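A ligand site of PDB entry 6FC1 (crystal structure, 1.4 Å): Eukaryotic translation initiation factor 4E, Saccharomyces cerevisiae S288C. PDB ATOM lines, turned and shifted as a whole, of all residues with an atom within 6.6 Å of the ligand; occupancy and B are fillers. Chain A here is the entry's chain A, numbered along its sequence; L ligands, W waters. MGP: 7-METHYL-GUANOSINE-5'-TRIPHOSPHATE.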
ATOM      1  N   TRP A  38       4.914  -3.403   2.546  1.00  0.00           N
ATOM      2  CA  TRP A  38       4.965  -3.124   1.118  1.00  0.00           C
ATOM      3  C   TRP A  38       5.755  -1.855   0.844  1.00  0.00           C
ATOM      4  O   TRP A  38       6.608  -1.838  -0.052  1.00  0.00           O
ATOM      5  CB  TRP A  38       3.528  -3.014   0.583  1.00  0.00           C
ATOM      6  CG  TRP A  38       3.433  -2.490  -0.825  1.00  0.00           C
ATOM      7  CD1 TRP A  38       3.118  -1.227  -1.182  1.00  0.00           C
ATOM      8  CD2 TRP A  38       3.676  -3.198  -2.035  1.00  0.00           C
ATOM      9  NE1 TRP A  38       3.133  -1.086  -2.525  1.00  0.00           N
ATOM     10  CE2 TRP A  38       3.468  -2.290  -3.096  1.00  0.00           C
ATOM     11  CE3 TRP A  38       4.027  -4.517  -2.344  1.00  0.00           C
ATOM     12  CZ2 TRP A  38       3.595  -2.651  -4.443  1.00  0.00           C
ATOM     13  CZ3 TRP A  38       4.165  -4.886  -3.667  1.00  0.00           C
ATOM     14  CH2 TRP A  38       3.961  -3.941  -4.710  1.00  0.00           C
ATOM     15  N   SER A  39       5.540  -0.798   1.637  1.00  0.00           N
ATOM     16  CA  SER A  39       6.206   0.468   1.399  1.00  0.00           C
ATOM     17  C   SER A  39       7.716   0.371   1.619  1.00  0.00           C
ATOM     18  O   SER A  39       8.460   1.134   1.037  1.00  0.00           O
ATOM     19  CB  SER A  39       5.623   1.565   2.302  1.00  0.00           C
ATOM     20  OG  SER A  39       4.266   1.832   1.973  1.00  0.00           O
ATOM     21  N   LYS A  70       8.209 -14.214  -3.824  1.00  0.00           N
ATOM     22  CA  LYS A  70       7.522 -13.020  -3.351  1.00  0.00           C
ATOM     23  C   LYS A  70       8.158 -11.730  -3.858  1.00  0.00           C
ATOM     24  O   LYS A  70       7.685 -10.632  -3.476  1.00  0.00           O
ATOM     25  CB  LYS A  70       7.313 -13.037  -1.830  1.00  0.00           C
ATOM     26  CG  LYS A  70       6.162 -13.909  -1.458  1.00  0.00           C
ATOM     27  CD  LYS A  70       4.832 -13.234  -1.815  1.00  0.00           C
ATOM     28  CE  LYS A  70       4.412 -12.184  -0.757  1.00  0.00           C
ATOM     29  NZ  LYS A  70       3.068 -11.605  -1.091  1.00  0.00           N
ATOM     30  N   ASP A  72       8.898  -9.053  -7.144  1.00  0.00           N
ATOM     31  CA  ASP A  72       8.260  -8.594  -8.375  1.00  0.00           C
ATOM     32  C   ASP A  72       9.243  -7.706  -9.126  1.00  0.00           C
ATOM     33  O   ASP A  72       9.977  -6.925  -8.527  1.00  0.00           O
ATOM     34  CB  ASP A  72       6.977  -7.708  -8.173  1.00  0.00           C
ATOM     35  CG  ASP A  72       5.895  -8.277  -7.263  1.00  0.00           C
ATOM     36  OD1 ASP A  72       5.314  -9.316  -7.601  1.00  0.00           O
ATOM     37  OD2 ASP A  72       5.525  -7.536  -6.317  1.00  0.00           O
ATOM     38  N   HIS A  74       8.592  -4.551 -11.834  1.00  0.00           N
ATOM     39  CA  HIS A  74       7.556  -3.699 -12.408  1.00  0.00           C
ATOM     40  C   HIS A  74       8.217  -2.731 -13.363  1.00  0.00           C
ATOM     41  O   HIS A  74       9.250  -2.136 -13.040  1.00  0.00           O
ATOM     42  CB  HIS A  74       6.833  -2.874 -11.329  1.00  0.00           C
ATOM     43  CG  HIS A  74       6.692  -3.510  -9.999  1.00  0.00           C
ATOM     44  ND1 HIS A  74       5.466  -3.842  -9.450  1.00  0.00           N
ATOM     45  CD2 HIS A  74       7.617  -3.809  -9.043  1.00  0.00           C
ATOM     46  CE1 HIS A  74       5.653  -4.312  -8.226  1.00  0.00           C
ATOM     47  NE2 HIS A  74       6.949  -4.318  -7.982  1.00  0.00           N
ATOM     48  N   PRO A  82       3.885   1.751  -9.280  1.00  0.00           N
ATOM     49  CA  PRO A  82       3.218   0.460  -9.579  1.00  0.00           C
ATOM     50  C   PRO A  82       2.282   0.004  -8.464  1.00  0.00           C
ATOM     51  O   PRO A  82       2.402  -1.094  -7.922  1.00  0.00           O
ATOM     52  CB  PRO A  82       4.430  -0.483  -9.784  1.00  0.00           C
ATOM     53  CG  PRO A  82       5.430   0.048  -8.777  1.00  0.00           C
ATOM     54  CD  PRO A  82       5.292   1.546  -8.857  1.00  0.00           C
ATOM     55  N   GLU A  83       1.318   0.867  -8.128  1.00  0.00           N
ATOM     56  CA  GLU A  83       0.469   0.737  -6.964  1.00  0.00           C
ATOM     57  C   GLU A  83      -0.954   1.098  -7.371  1.00  0.00           C
ATOM     58  O   GLU A  83      -1.169   2.045  -8.136  1.00  0.00           O
ATOM     59  CB  GLU A  83       0.929   1.724  -5.868  1.00  0.00           C
ATOM     60  CG  GLU A  83       2.237   1.333  -5.316  1.00  0.00           C
ATOM     61  CD  GLU A  83       2.685   2.248  -4.213  1.00  0.00           C
ATOM     62  OE1 GLU A  83       2.514   3.496  -4.309  1.00  0.00           O
ATOM     63  OE2 GLU A  83       3.114   1.695  -3.209  1.00  0.00           O
ATOM     64  N   TRP A  84      -1.928   0.364  -6.801  1.00  0.00           N
ATOM     65  CA  TRP A  84      -3.330   0.635  -7.060  1.00  0.00           C
ATOM     66  C   TRP A  84      -3.732   2.037  -6.607  1.00  0.00           C
ATOM     67  O   TRP A  84      -4.695   2.606  -7.149  1.00  0.00           O
ATOM     68  CB  TRP A  84      -4.182  -0.361  -6.272  1.00  0.00           C
ATOM     69  CG  TRP A  84      -3.723  -1.811  -6.188  1.00  0.00           C
ATOM     70  CD1 TRP A  84      -3.427  -2.620  -7.228  1.00  0.00           C
ATOM     71  CD2 TRP A  84      -3.560  -2.602  -4.998  1.00  0.00           C
ATOM     72  NE1 TRP A  84      -3.066  -3.872  -6.775  1.00  0.00           N
ATOM     73  CE2 TRP A  84      -3.143  -3.891  -5.407  1.00  0.00           C
ATOM     74  CE3 TRP A  84      -3.711  -2.353  -3.643  1.00  0.00           C
ATOM     75  CZ2 TRP A  84      -2.850  -4.905  -4.512  1.00  0.00           C
ATOM     76  CZ3 TRP A  84      -3.433  -3.375  -2.744  1.00  0.00           C
ATOM     77  CH2 TRP A  84      -3.028  -4.633  -3.187  1.00  0.00           C
ATOM     78  N   GLU A  85      -3.032   2.597  -5.596  1.00  0.00           N
ATOM     79  CA  GLU A  85      -3.321   3.939  -5.074  1.00  0.00           C
ATOM     80  C   GLU A  85      -2.860   5.064  -5.989  1.00  0.00           C
ATOM     81  O   GLU A  85      -3.263   6.220  -5.789  1.00  0.00           O
ATOM     82  CB  GLU A  85      -2.601   4.130  -3.739  1.00  0.00           C
ATOM     83  CG  GLU A  85      -3.059   3.254  -2.635  1.00  0.00           C
ATOM     84  CD  GLU A  85      -2.108   2.131  -2.406  1.00  0.00           C
ATOM     85  OE1 GLU A  85      -1.628   1.557  -3.404  1.00  0.00           O
ATOM     86  OE2 GLU A  85      -1.839   1.821  -1.224  1.00  0.00           O
ATOM     87  N   LYS A  94      -5.852  -4.873 -13.883  1.00  0.00           N
ATOM     88  CA  LYS A  94      -4.779  -5.612 -14.549  1.00  0.00           C
ATOM     89  C   LYS A  94      -5.294  -6.842 -15.257  1.00  0.00           C
ATOM     90  O   LYS A  94      -6.131  -7.574 -14.728  1.00  0.00           O
ATOM     91  CB  LYS A  94      -3.620  -6.026 -13.571  1.00  0.00           C
ATOM     92  CG  LYS A  94      -4.041  -6.985 -12.453  1.00  0.00           C
ATOM     93  CD  LYS A  94      -2.860  -7.298 -11.484  1.00  0.00           C
ATOM     94  CE  LYS A  94      -3.274  -8.347 -10.485  1.00  0.00           C
ATOM     95  NZ  LYS A  94      -2.122  -8.761  -9.640  1.00  0.00           N
ATOM     96  N   SER A 135       5.502 -11.291 -11.262  1.00  0.00           N
ATOM     97  CA  SER A 135       5.385 -11.667  -9.853  1.00  0.00           C
ATOM     98  C   SER A 135       5.826 -13.103  -9.676  1.00  0.00           C
ATOM     99  O   SER A 135       5.275 -14.019 -10.309  1.00  0.00           O
ATOM    100  CB  SER A 135       3.921 -11.541  -9.409  1.00  0.00           C
ATOM    101  OG  SER A 135       3.467 -10.219  -9.487  1.00  0.00           O
ATOM    102  N   ARG A 137       5.846 -16.305  -7.487  1.00  0.00           N
ATOM    103  CA  ARG A 137       4.939 -16.820  -6.467  1.00  0.00           C
ATOM    104  C   ARG A 137       4.997 -18.339  -6.455  1.00  0.00           C
ATOM    105  O   ARG A 137       5.153 -18.984  -7.495  1.00  0.00           O
ATOM    106  CB  ARG A 137       3.484 -16.381  -6.724  1.00  0.00           C
ATOM    107  CG  ARG A 137       3.278 -14.907  -6.726  1.00  0.00           C
ATOM    108  CD  ARG A 137       3.499 -14.284  -5.375  1.00  0.00           C
ATOM    109  NE  ARG A 137       3.078 -12.870  -5.471  1.00  0.00           N
ATOM    110  CZ  ARG A 137       3.873 -11.873  -5.793  1.00  0.00           C
ATOM    111  NH1 ARG A 137       5.158 -12.070  -6.037  1.00  0.00           N
ATOM    112  NH2 ARG A 137       3.360 -10.655  -5.911  1.00  0.00           N
ATOM    113  N   LYS A 138       4.823 -18.916  -5.261  1.00  0.00           N
ATOM    114  CA  LYS A 138       4.939 -20.362  -5.074  1.00  0.00           C
ATOM    115  C   LYS A 138       3.990 -21.133  -5.986  1.00  0.00           C
ATOM    116  O   LYS A 138       4.337 -22.209  -6.490  1.00  0.00           O
ATOM    117  CB  LYS A 138       4.663 -20.719  -3.606  1.00  0.00           C
ATOM    118  CG  LYS A 138       5.015 -22.166  -3.249  1.00  0.00           C
ATOM    119  CD  LYS A 138       4.171 -22.671  -2.094  1.00  0.00           C
ATOM    120  CE  LYS A 138       4.341 -24.182  -1.895  1.00  0.00           C
ATOM    121  NZ  LYS A 138       3.567 -24.677  -0.710  1.00  0.00           N
ATOM    122  N   LYS A 142       3.433 -14.988 -12.323  1.00  0.00           N
ATOM    123  CA  LYS A 142       2.377 -14.238 -12.984  1.00  0.00           C
ATOM    124  C   LYS A 142       2.942 -13.101 -13.812  1.00  0.00           C
ATOM    125  O   LYS A 142       3.917 -12.436 -13.426  1.00  0.00           O
ATOM    126  CB  LYS A 142       1.371 -13.657 -11.955  1.00  0.00           C
ATOM    127  CG  LYS A 142       0.795 -14.688 -11.073  1.00  0.00           C
ATOM    128  CD  LYS A 142      -0.261 -14.138 -10.145  1.00  0.00           C
ATOM    129  CE  LYS A 142       0.280 -13.178  -9.140  1.00  0.00           C
ATOM    130  NZ  LYS A 142      -0.781 -12.715  -8.237  1.00  0.00           N
ATOM    131  N   TRP A 146      -0.983  -3.620 -16.443  1.00  0.00           N
ATOM    132  CA  TRP A 146      -1.787  -2.680 -15.663  1.00  0.00           C
ATOM    133  C   TRP A 146      -2.327  -1.583 -16.568  1.00  0.00           C
ATOM    134  O   TRP A 146      -1.568  -0.930 -17.279  1.00  0.00           O
ATOM    135  CB  TRP A 146      -0.914  -2.083 -14.555  1.00  0.00           C
ATOM    136  CG  TRP A 146      -0.693  -2.980 -13.368  1.00  0.00           C
ATOM    137  CD1 TRP A 146      -0.380  -4.333 -13.351  1.00  0.00           C
ATOM    138  CD2 TRP A 146      -0.849  -2.586 -12.005  1.00  0.00           C
ATOM    139  NE1 TRP A 146      -0.359  -4.787 -12.049  1.00  0.00           N
ATOM    140  CE2 TRP A 146      -0.581  -3.729 -11.205  1.00  0.00           C
ATOM    141  CE3 TRP A 146      -1.083  -1.374 -11.372  1.00  0.00           C
ATOM    142  CZ2 TRP A 146      -0.637  -3.676  -9.807  1.00  0.00           C
ATOM    143  CZ3 TRP A 146      -1.108  -1.330 -10.007  1.00  0.00           C
ATOM    144  CH2 TRP A 146      -0.862  -2.473  -9.236  1.00  0.00           C
HETATM  145  PA  MGP L   1      -0.231  -8.798  -4.633  1.00  0.00           P
HETATM  146  O1A MGP L   1      -1.189  -7.959  -5.406  1.00  0.00           O
HETATM  147  O2A MGP L   1       1.024  -9.018  -5.304  1.00  0.00           O
HETATM  148  O3A MGP L   1      -0.912 -10.149  -4.327  1.00  0.00           O
HETATM  149  O5' MGP L   1      -0.220  -8.077  -3.201  1.00  0.00           O
HETATM  150  PB  MGP L   1      -0.588 -11.635  -4.660  1.00  0.00           P
HETATM  151  O1B MGP L   1      -1.915 -12.277  -4.967  1.00  0.00           O
HETATM  152  O2B MGP L   1       0.433 -11.846  -5.717  1.00  0.00           O
HETATM  153  O3B MGP L   1      -0.053 -12.125  -3.290  1.00  0.00           O
HETATM  154  PC  MGP L   1       0.114 -13.577  -2.791  1.00  0.00           P
HETATM  155  O1C MGP L   1       1.368 -13.556  -1.885  1.00  0.00           O
HETATM  156  O2C MGP L   1       0.266 -14.598  -3.875  1.00  0.00           O
HETATM  157  O3C MGP L   1      -1.186 -13.907  -1.911  1.00  0.00           O
HETATM  158  C5' MGP L   1       0.208  -8.728  -1.994  1.00  0.00           C
HETATM  159  C4' MGP L   1       0.214  -7.667  -0.862  1.00  0.00           C
HETATM  160  O4' MGP L   1       1.252  -6.685  -1.198  1.00  0.00           O
HETATM  161  C3' MGP L   1      -1.158  -6.899  -0.658  1.00  0.00           C
HETATM  162  O3' MGP L   1      -1.886  -7.380   0.470  1.00  0.00           O
HETATM  163  C2' MGP L   1      -0.689  -5.583  -0.153  1.00  0.00           C
HETATM  164  O2' MGP L   1      -0.563  -5.820   1.210  1.00  0.00           O
HETATM  165  C1' MGP L   1       0.735  -5.440  -0.824  1.00  0.00           C
HETATM  166  N9  MGP L   1       0.521  -4.721  -2.110  1.00  0.00           N
HETATM  167  C8  MGP L   1       0.776  -5.189  -3.378  1.00  0.00           C
HETATM  168  N7  MGP L   1       0.484  -4.199  -4.265  1.00  0.00           N
HETATM  169  CM7 MGP L   1       0.623  -4.248  -5.705  1.00  0.00           C
HETATM  170  C5  MGP L   1       0.035  -3.097  -3.548  1.00  0.00           C
HETATM  171  C6  MGP L   1      -0.382  -1.816  -3.944  1.00  0.00           C
HETATM  172  O6  MGP L   1      -0.513  -1.396  -5.087  1.00  0.00           O
HETATM  173  N1  MGP L   1      -0.740  -0.991  -2.872  1.00  0.00           N
HETATM  174  C2  MGP L   1      -0.675  -1.401  -1.569  1.00  0.00           C
HETATM  175  N2  MGP L   1      -1.059  -0.500  -0.670  1.00  0.00           N
HETATM  176  N3  MGP L   1      -0.262  -2.625  -1.145  1.00  0.00           N
HETATM  177  C4  MGP L   1       0.072  -3.435  -2.170  1.00  0.00           C
HETATM  178  O   HOH W   1      -4.050  -8.516  -5.627  1.00  0.00           O
HETATM  179  O   HOH W   2       2.752  -7.285  -6.355  1.00  0.00           O
HETATM  180  O   HOH W   3       0.033  -3.170   1.990  1.00  0.00           O
HETATM  181  O   HOH W   4       1.460  -6.118  -8.517  1.00  0.00           O
HETATM  182  O   HOH W   5      -3.047 -10.688  -7.851  1.00  0.00           O
HETATM  183  O   HOH W   6       0.693 -15.272   0.695  1.00  0.00           O
HETATM  184  O   HOH W   7      -2.539 -10.218   0.531  1.00  0.00           O
HETATM  185  O   HOH W   8       0.595  -9.927  -8.267  1.00  0.00           O
HETATM  186  O   HOH W   9      -1.201  -6.722  -7.829  1.00  0.00           O
HETATM  187  O   HOH W  10      -0.535 -15.069  -6.402  1.00  0.00           O
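The side-chain carboxylate (OE2) of Glu 85 is in hydrogen-bond range of a nitrogen (N2) of the ligand. An oxygen (O1C) of the ligand lies within salt-bridge range of the side-chain amino group of Lys 70, 2.7 Å away. O6 of the ligand sits at hydrogen-bond distance from N of Trp 84 (2.8 Å). An oxygen (O2B) of the ligand lies within salt-bridge range of the guanidinium group (NE) of Arg 137 (2.8 Å). NZ of Lys 142 is in salt-bridge range of O2B of the ligand (2.9 Å).
NH2 of Arg 137 lies within salt-bridge range of OD1 of Asp 72 (2.9 Å). The backbone carbonyl oxygen (O) of Ser 135 is in hydrogen-bond range of the backbone NH (N) of Lys 142 (2.9 Å). OE2 of Glu 83 sits at hydrogen-bond distance from NE1 of Trp 38, at 2.9 Å.
Water W2 lies within hydrogen-bond range of O2A of the ligand, OD2 of Asp 72 and NH2 of Arg 137. Water W10 lies within hydrogen-bond range of O2C of the ligand and NZ of Lys 142. Water W9 bridges an oxygen (O1A) of the ligand and the side-chain amino group (NZ) of Lys 94. Water W8 lies within hydrogen-bond range of NZ of Lys 142, O2A of the ligand, OG of Ser 135 and NZ of Lys 94. Water W5 lies within hydrogen-bond range of NZ of Lys 94 (2.8 Å), NZ of Lys 142 (3.1 Å) and O1B of the ligand (3.5 Å).
Residues that only touch the ligand: Glu 83 and Trp 38. Hydrophobic or aromatic side chains within 4 Å of the ligand: Trp 38 and Trp 84. Of the 15 residues printed, 7 come within 4 Å of the ligand.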
